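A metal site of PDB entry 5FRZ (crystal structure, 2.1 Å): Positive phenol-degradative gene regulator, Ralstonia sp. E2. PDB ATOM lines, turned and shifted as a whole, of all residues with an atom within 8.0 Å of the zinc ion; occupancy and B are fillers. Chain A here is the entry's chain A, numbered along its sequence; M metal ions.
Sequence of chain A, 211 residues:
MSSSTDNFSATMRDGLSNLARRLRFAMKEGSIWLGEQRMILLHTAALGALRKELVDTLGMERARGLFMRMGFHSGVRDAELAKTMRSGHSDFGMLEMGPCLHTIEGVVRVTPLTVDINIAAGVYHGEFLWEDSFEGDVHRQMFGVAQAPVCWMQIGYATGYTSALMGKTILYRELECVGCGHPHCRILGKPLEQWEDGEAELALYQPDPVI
The side-chain sulfur (SG) of Cys 185 lies close to the backbone NH (N) of Val 178, at 3.5 Å. The side-chain sulfur (SG) of Cys 185 sits close to the side-chain hydroxyl (OG) of Ser 133. N of Val 150 sits at hydrogen-bond distance from OE1 of Glu 174 (3.4 Å). The backbone NH (N) of Val 150 sits close to the side-chain sulfur (SG) of Cys 177 (3.3 Å). O of Cys 185 lies within hydrogen-bond range of N of Trp 130 (2.8 Å). The side-chain sulfur of Cys 177 lies close to the backbone NH of Gly 179, 3.3 Å away. SG of Cys 151 sits close to N of Gly 136 (3.4 Å).
The nearest printed residue that does not touch the zinc ion is Val 178 (4.1 Å).
The zinc ion is bound by OE2 of Glu 174 (2.1 Å), SG of Cys 185 (2.2 Å), SG of Cys 151 (2.3 Å) and SG of Cys 177 (2.4 Å).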
ATOM      1  N   VAL A 108      -2.300  22.191  13.120  1.00  0.00           N
ATOM      2  CA  VAL A 108      -3.223  23.299  12.882  1.00  0.00           C
ATOM      3  C   VAL A 108      -4.589  22.911  13.434  1.00  0.00           C
ATOM      4  O   VAL A 108      -4.877  21.717  13.591  1.00  0.00           O
ATOM      5  CB  VAL A 108      -3.335  23.642  11.359  1.00  0.00           C
ATOM      6  CG1 VAL A 108      -4.004  22.488  10.579  1.00  0.00           C
ATOM      7  CG2 VAL A 108      -4.087  24.948  11.124  1.00  0.00           C
ATOM      8  N   TRP A 130      -7.883  27.899   8.932  1.00  0.00           N
ATOM      9  CA  TRP A 130      -6.761  27.358   9.687  1.00  0.00           C
ATOM     10  C   TRP A 130      -6.379  28.340  10.769  1.00  0.00           C
ATOM     11  O   TRP A 130      -6.053  29.490  10.487  1.00  0.00           O
ATOM     12  CB  TRP A 130      -5.563  27.108   8.788  1.00  0.00           C
ATOM     13  CG  TRP A 130      -5.551  25.770   8.089  1.00  0.00           C
ATOM     14  CD1 TRP A 130      -6.306  24.677   8.387  1.00  0.00           C
ATOM     15  CD2 TRP A 130      -4.728  25.426   6.987  1.00  0.00           C
ATOM     16  NE1 TRP A 130      -5.996  23.648   7.511  1.00  0.00           N
ATOM     17  CE2 TRP A 130      -5.026  24.079   6.647  1.00  0.00           C
ATOM     18  CE3 TRP A 130      -3.760  26.111   6.246  1.00  0.00           C
ATOM     19  CZ2 TRP A 130      -4.389  23.421   5.610  1.00  0.00           C
ATOM     20  CZ3 TRP A 130      -3.124  25.441   5.203  1.00  0.00           C
ATOM     21  CH2 TRP A 130      -3.449  24.120   4.890  1.00  0.00           C
ATOM     22  N   SER A 133      -1.758  27.710  12.816  1.00  0.00           N
ATOM     23  CA  SER A 133      -0.881  27.003  11.893  1.00  0.00           C
ATOM     24  C   SER A 133       0.551  26.934  12.418  1.00  0.00           C
ATOM     25  O   SER A 133       1.185  27.969  12.611  1.00  0.00           O
ATOM     26  CB  SER A 133      -0.871  27.690  10.528  1.00  0.00           C
ATOM     27  OG  SER A 133      -2.111  27.542   9.840  1.00  0.00           O
ATOM     28  N   PHE A 134       1.068  25.726  12.638  1.00  0.00           N
ATOM     29  CA  PHE A 134       2.440  25.618  13.117  1.00  0.00           C
ATOM     30  C   PHE A 134       3.348  26.201  12.059  1.00  0.00           C
ATOM     31  O   PHE A 134       4.312  26.890  12.378  1.00  0.00           O
ATOM     32  CB  PHE A 134       2.845  24.168  13.410  1.00  0.00           C
ATOM     33  CG  PHE A 134       3.562  23.482  12.278  1.00  0.00           C
ATOM     34  CD1 PHE A 134       4.933  23.622  12.114  1.00  0.00           C
ATOM     35  CD2 PHE A 134       2.849  22.698  11.372  1.00  0.00           C
ATOM     36  CE1 PHE A 134       5.588  23.026  11.059  1.00  0.00           C
ATOM     37  CE2 PHE A 134       3.497  22.087  10.317  1.00  0.00           C
ATOM     38  CZ  PHE A 134       4.873  22.244  10.167  1.00  0.00           C
ATOM     39  N   GLU A 135       3.039  25.926  10.788  1.00  0.00           N
ATOM     40  CA  GLU A 135       3.973  26.163   9.703  1.00  0.00           C
ATOM     41  C   GLU A 135       4.093  27.643   9.370  1.00  0.00           C
ATOM     42  O   GLU A 135       5.193  28.156   9.083  1.00  0.00           O
ATOM     43  CB  GLU A 135       3.555  25.377   8.465  1.00  0.00           C
ATOM     44  CG  GLU A 135       4.591  25.305   7.404  1.00  0.00           C
ATOM     45  CD  GLU A 135       4.193  24.372   6.269  1.00  0.00           C
ATOM     46  OE1 GLU A 135       2.995  24.018   6.177  1.00  0.00           O
ATOM     47  OE2 GLU A 135       5.074  24.007   5.446  1.00  0.00           O
ATOM     48  N   GLY A 136       2.957  28.334   9.392  1.00  0.00           N
ATOM     49  CA  GLY A 136       2.932  29.771   9.227  1.00  0.00           C
ATOM     50  C   GLY A 136       3.684  30.447  10.368  1.00  0.00           C
ATOM     51  O   GLY A 136       4.544  31.301  10.145  1.00  0.00           O
ATOM     52  N   ASP A 137       3.377  30.035  11.586  1.00  0.00           N
ATOM     53  CA  ASP A 137       4.014  30.594  12.763  1.00  0.00           C
ATOM     54  C   ASP A 137       5.532  30.454  12.696  1.00  0.00           C
ATOM     55  O   ASP A 137       6.250  31.411  12.968  1.00  0.00           O
ATOM     56  CB  ASP A 137       3.463  29.952  14.037  1.00  0.00           C
ATOM     57  CG  ASP A 137       1.978  30.262  14.276  1.00  0.00           C
ATOM     58  OD1 ASP A 137       1.253  30.615  13.301  1.00  0.00           O
ATOM     59  OD2 ASP A 137       1.544  30.153  15.451  1.00  0.00           O
ATOM     60  N   ALA A 148       4.003  35.524  -0.247  1.00  0.00           N
ATOM     61  CA  ALA A 148       2.894  34.617  -0.560  1.00  0.00           C
ATOM     62  C   ALA A 148       2.680  33.595   0.575  1.00  0.00           C
ATOM     63  O   ALA A 148       3.626  33.337   1.350  1.00  0.00           O
ATOM     64  CB  ALA A 148       3.157  33.904  -1.885  1.00  0.00           C
ATOM     65  N   PRO A 149       1.456  33.038   0.691  1.00  0.00           N
ATOM     66  CA  PRO A 149       1.149  32.009   1.695  1.00  0.00           C
ATOM     67  C   PRO A 149       2.260  30.990   1.881  1.00  0.00           C
ATOM     68  O   PRO A 149       2.931  30.647   0.903  1.00  0.00           O
ATOM     69  CB  PRO A 149      -0.108  31.346   1.128  1.00  0.00           C
ATOM     70  CG  PRO A 149      -0.826  32.482   0.430  1.00  0.00           C
ATOM     71  CD  PRO A 149       0.260  33.410  -0.098  1.00  0.00           C
ATOM     72  N   VAL A 150       2.461  30.506   3.097  1.00  0.00           N
ATOM     73  CA  VAL A 150       3.643  29.677   3.409  1.00  0.00           C
ATOM     74  C   VAL A 150       3.383  28.307   4.069  1.00  0.00           C
ATOM     75  O   VAL A 150       4.320  27.600   4.396  1.00  0.00           O
ATOM     76  CB  VAL A 150       4.599  30.450   4.345  1.00  0.00           C
ATOM     77  CG1 VAL A 150       5.325  31.531   3.567  1.00  0.00           C
ATOM     78  CG2 VAL A 150       3.846  31.018   5.534  1.00  0.00           C
ATOM     79  N   CYS A 151       2.131  27.914   4.218  1.00  0.00           N
ATOM     80  CA  CYS A 151       1.846  26.648   4.889  1.00  0.00           C
ATOM     81  C   CYS A 151       1.862  25.501   3.877  1.00  0.00           C
ATOM     82  O   CYS A 151       0.868  24.820   3.660  1.00  0.00           O
ATOM     83  CB  CYS A 151       0.527  26.755   5.666  1.00  0.00           C
ATOM     84  SG  CYS A 151       0.633  28.082   6.957  1.00  0.00           S
ATOM     85  N   TRP A 152       3.051  25.311   3.305  1.00  0.00           N
ATOM     86  CA  TRP A 152       3.332  24.358   2.231  1.00  0.00           C
ATOM     87  C   TRP A 152       3.046  22.906   2.594  1.00  0.00           C
ATOM     88  O   TRP A 152       2.332  22.212   1.882  1.00  0.00           O
ATOM     89  CB  TRP A 152       4.803  24.480   1.829  1.00  0.00           C
ATOM     90  CG  TRP A 152       5.229  25.885   1.461  1.00  0.00           C
ATOM     91  CD1 TRP A 152       4.444  26.865   0.919  1.00  0.00           C
ATOM     92  CD2 TRP A 152       6.542  26.431   1.602  1.00  0.00           C
ATOM     93  NE1 TRP A 152       5.197  28.004   0.725  1.00  0.00           N
ATOM     94  CE2 TRP A 152       6.487  27.770   1.126  1.00  0.00           C
ATOM     95  CE3 TRP A 152       7.750  25.939   2.093  1.00  0.00           C
ATOM     96  CZ2 TRP A 152       7.601  28.606   1.120  1.00  0.00           C
ATOM     97  CZ3 TRP A 152       8.864  26.775   2.087  1.00  0.00           C
ATOM     98  CH2 TRP A 152       8.780  28.097   1.599  1.00  0.00           C
ATOM     99  N   GLN A 154       1.295  21.942   5.148  1.00  0.00           N
ATOM    100  CA  GLN A 154      -0.117  21.867   5.529  1.00  0.00           C
ATOM    101  C   GLN A 154      -1.045  21.782   4.315  1.00  0.00           C
ATOM    102  O   GLN A 154      -2.025  21.025   4.330  1.00  0.00           O
ATOM    103  CB  GLN A 154      -0.513  23.047   6.403  1.00  0.00           C
ATOM    104  CG  GLN A 154       0.289  23.133   7.689  1.00  0.00           C
ATOM    105  CD  GLN A 154      -0.141  24.276   8.625  1.00  0.00           C
ATOM    106  OE1 GLN A 154       0.576  24.613   9.554  1.00  0.00           O
ATOM    107  NE2 GLN A 154      -1.314  24.865   8.379  1.00  0.00           N
ATOM    108  N   ILE A 155      -0.739  22.538   3.262  1.00  0.00           N
ATOM    109  CA  ILE A 155      -1.522  22.487   2.035  1.00  0.00           C
ATOM    110  C   ILE A 155      -1.391  21.126   1.331  1.00  0.00           C
ATOM    111  O   ILE A 155      -2.391  20.542   0.904  1.00  0.00           O
ATOM    112  CB  ILE A 155      -1.095  23.603   1.057  1.00  0.00           C
ATOM    113  CG1 ILE A 155      -1.882  24.863   1.381  1.00  0.00           C
ATOM    114  CG2 ILE A 155      -1.387  23.198  -0.422  1.00  0.00           C
ATOM    115  CD1 ILE A 155      -3.391  24.755   1.041  1.00  0.00           C
ATOM    116  N   GLU A 174      -4.023  28.191  -0.451  1.00  0.00           N
ATOM    117  CA  GLU A 174      -4.222  29.147   0.612  1.00  0.00           C
ATOM    118  C   GLU A 174      -4.614  30.508   0.054  1.00  0.00           C
ATOM    119  O   GLU A 174      -3.832  31.108  -0.663  1.00  0.00           O
ATOM    120  CB  GLU A 174      -2.942  29.299   1.427  1.00  0.00           C
ATOM    121  CG  GLU A 174      -2.643  28.211   2.378  1.00  0.00           C
ATOM    122  CD  GLU A 174      -1.575  28.618   3.361  1.00  0.00           C
ATOM    123  OE1 GLU A 174      -0.378  28.558   2.995  1.00  0.00           O
ATOM    124  OE2 GLU A 174      -1.927  29.033   4.473  1.00  0.00           O
ATOM    125  N   LEU A 175      -5.790  31.007   0.410  1.00  0.00           N
ATOM    126  CA  LEU A 175      -6.235  32.337  -0.025  1.00  0.00           C
ATOM    127  C   LEU A 175      -5.813  33.389   0.985  1.00  0.00           C
ATOM    128  O   LEU A 175      -5.806  34.589   0.709  1.00  0.00           O
ATOM    129  CB  LEU A 175      -7.756  32.363  -0.201  1.00  0.00           C
ATOM    130  CG  LEU A 175      -8.373  31.123  -0.878  1.00  0.00           C
ATOM    131  CD1 LEU A 175      -9.885  31.249  -1.034  1.00  0.00           C
ATOM    132  CD2 LEU A 175      -7.701  30.841  -2.229  1.00  0.00           C
ATOM    133  N   GLU A 176      -5.454  32.908   2.173  1.00  0.00           N
ATOM    134  CA  GLU A 176      -5.065  33.742   3.288  1.00  0.00           C
ATOM    135  C   GLU A 176      -4.039  32.977   4.112  1.00  0.00           C
ATOM    136  O   GLU A 176      -4.113  31.749   4.163  1.00  0.00           O
ATOM    137  CB  GLU A 176      -6.284  34.095   4.134  1.00  0.00           C
ATOM    138  CG  GLU A 176      -6.486  35.571   4.215  1.00  0.00           C
ATOM    139  CD  GLU A 176      -7.893  35.978   4.461  1.00  0.00           C
ATOM    140  OE1 GLU A 176      -8.426  35.615   5.532  1.00  0.00           O
ATOM    141  OE2 GLU A 176      -8.446  36.690   3.596  1.00  0.00           O
ATOM    142  N   CYS A 177      -3.097  33.675   4.754  1.00  0.00           N
ATOM    143  CA  CYS A 177      -2.058  32.988   5.542  1.00  0.00           C
ATOM    144  C   CYS A 177      -1.387  33.864   6.589  1.00  0.00           C
ATOM    145  O   CYS A 177      -0.891  34.937   6.261  1.00  0.00           O
ATOM    146  CB  CYS A 177      -0.966  32.428   4.609  1.00  0.00           C
ATOM    147  SG  CYS A 177       0.333  31.474   5.461  1.00  0.00           S
ATOM    148  N   VAL A 178      -1.356  33.384   7.837  1.00  0.00           N
ATOM    149  CA  VAL A 178      -0.661  34.097   8.915  1.00  0.00           C
ATOM    150  C   VAL A 178       0.779  34.451   8.552  1.00  0.00           C
ATOM    151  O   VAL A 178       1.314  35.463   9.002  1.00  0.00           O
ATOM    152  CB  VAL A 178      -0.640  33.289  10.235  1.00  0.00           C
ATOM    153  CG1 VAL A 178      -1.980  33.356  10.932  1.00  0.00           C
ATOM    154  CG2 VAL A 178      -0.206  31.842   9.994  1.00  0.00           C
ATOM    155  N   GLY A 179       1.435  33.618   7.744  1.00  0.00           N
ATOM    156  CA  GLY A 179       2.803  33.885   7.352  1.00  0.00           C
ATOM    157  C   GLY A 179       2.907  35.164   6.527  1.00  0.00           C
ATOM    158  O   GLY A 179       4.005  35.678   6.291  1.00  0.00           O
ATOM    159  N   CYS A 180       1.749  35.662   6.105  1.00  0.00           N
ATOM    160  CA  CYS A 180       1.647  36.885   5.325  1.00  0.00           C
ATOM    161  C   CYS A 180       1.206  38.154   6.089  1.00  0.00           C
ATOM    162  O   CYS A 180       1.329  39.263   5.566  1.00  0.00           O
ATOM    163  CB  CYS A 180       0.681  36.656   4.155  1.00  0.00           C
ATOM    164  SG  CYS A 180       1.331  35.563   2.878  1.00  0.00           S
ATOM    165  N   HIS A 182      -1.723  38.101   7.884  1.00  0.00           N
ATOM    166  CA  HIS A 182      -3.088  37.631   8.036  1.00  0.00           C
ATOM    167  C   HIS A 182      -3.364  37.129   9.484  1.00  0.00           C
ATOM    168  O   HIS A 182      -2.465  36.616  10.139  1.00  0.00           O
ATOM    169  CB  HIS A 182      -3.225  36.565   6.957  1.00  0.00           C
ATOM    170  CG  HIS A 182      -3.065  37.090   5.551  1.00  0.00           C
ATOM    171  ND1 HIS A 182      -4.172  37.245   4.720  1.00  0.00           N
ATOM    172  CD2 HIS A 182      -2.065  37.834   5.001  1.00  0.00           C
ATOM    173  CE1 HIS A 182      -3.795  37.827   3.602  1.00  0.00           C
ATOM    174  NE2 HIS A 182      -2.509  38.238   3.752  1.00  0.00           N
ATOM    175  N   HIS A 184      -5.069  34.691  10.332  1.00  0.00           N
ATOM    176  CA  HIS A 184      -5.406  33.283  10.210  1.00  0.00           C
ATOM    177  C   HIS A 184      -5.164  32.831   8.777  1.00  0.00           C
ATOM    178  O   HIS A 184      -4.900  33.653   7.903  1.00  0.00           O
ATOM    179  CB  HIS A 184      -6.864  33.043  10.614  1.00  0.00           C
ATOM    180  CG  HIS A 184      -7.824  33.941   9.886  1.00  0.00           C
ATOM    181  ND1 HIS A 184      -8.251  33.690   8.620  1.00  0.00           N
ATOM    182  CD2 HIS A 184      -8.342  35.137  10.253  1.00  0.00           C
ATOM    183  CE1 HIS A 184      -9.047  34.688   8.227  1.00  0.00           C
ATOM    184  NE2 HIS A 184      -9.116  35.563   9.206  1.00  0.00           N
ATOM    185  N   CYS A 185      -5.259  31.525   8.539  1.00  0.00           N
ATOM    186  CA  CYS A 185      -5.153  30.981   7.194  1.00  0.00           C
ATOM    187  C   CYS A 185      -6.534  30.584   6.712  1.00  0.00           C
ATOM    188  O   CYS A 185      -7.410  30.268   7.527  1.00  0.00           O
ATOM    189  CB  CYS A 185      -4.210  29.772   7.156  1.00  0.00           C
ATOM    190  SG  CYS A 185      -2.470  30.037   7.738  1.00  0.00           S
ATOM    191  N   ARG A 186      -6.729  30.629   5.402  1.00  0.00           N
ATOM    192  CA  ARG A 186      -7.959  30.201   4.763  1.00  0.00           C
ATOM    193  C   ARG A 186      -7.645  29.461   3.460  1.00  0.00           C
ATOM    194  O   ARG A 186      -6.848  29.917   2.632  1.00  0.00           O
ATOM    195  CB  ARG A 186      -8.882  31.376   4.465  1.00  0.00           C
ATOM    196  CG  ARG A 186     -10.337  31.082   4.781  1.00  0.00           C
ATOM    197  CD  ARG A 186     -11.303  32.101   4.147  1.00  0.00           C
ATOM    198  NE  ARG A 186     -10.869  33.489   4.324  1.00  0.00           N
ATOM    199  CZ  ARG A 186     -11.085  34.218   5.424  1.00  0.00           C
ATOM    200  NH1 ARG A 186     -11.724  33.709   6.479  1.00  0.00           N
ATOM    201  NH2 ARG A 186     -10.649  35.476   5.478  1.00  0.00           N
ATOM    202  N   ILE A 187      -8.290  28.308   3.271  1.00  0.00           N
ATOM    203  CA  ILE A 187      -7.955  27.431   2.165  1.00  0.00           C
ATOM    204  C   ILE A 187      -9.166  27.054   1.313  1.00  0.00           C
ATOM    205  O   ILE A 187     -10.303  27.054   1.787  1.00  0.00           O
ATOM    206  CB  ILE A 187      -7.265  26.142   2.655  1.00  0.00           C
ATOM    207  CG1 ILE A 187      -8.283  25.230   3.351  1.00  0.00           C
ATOM    208  CG2 ILE A 187      -6.122  26.483   3.591  1.00  0.00           C
ATOM    209  CD1 ILE A 187      -7.674  23.917   3.861  1.00  0.00           C
HETATM  210 ZN    ZN M   1      -0.905  29.613   6.201  1.00  0.00          ZN
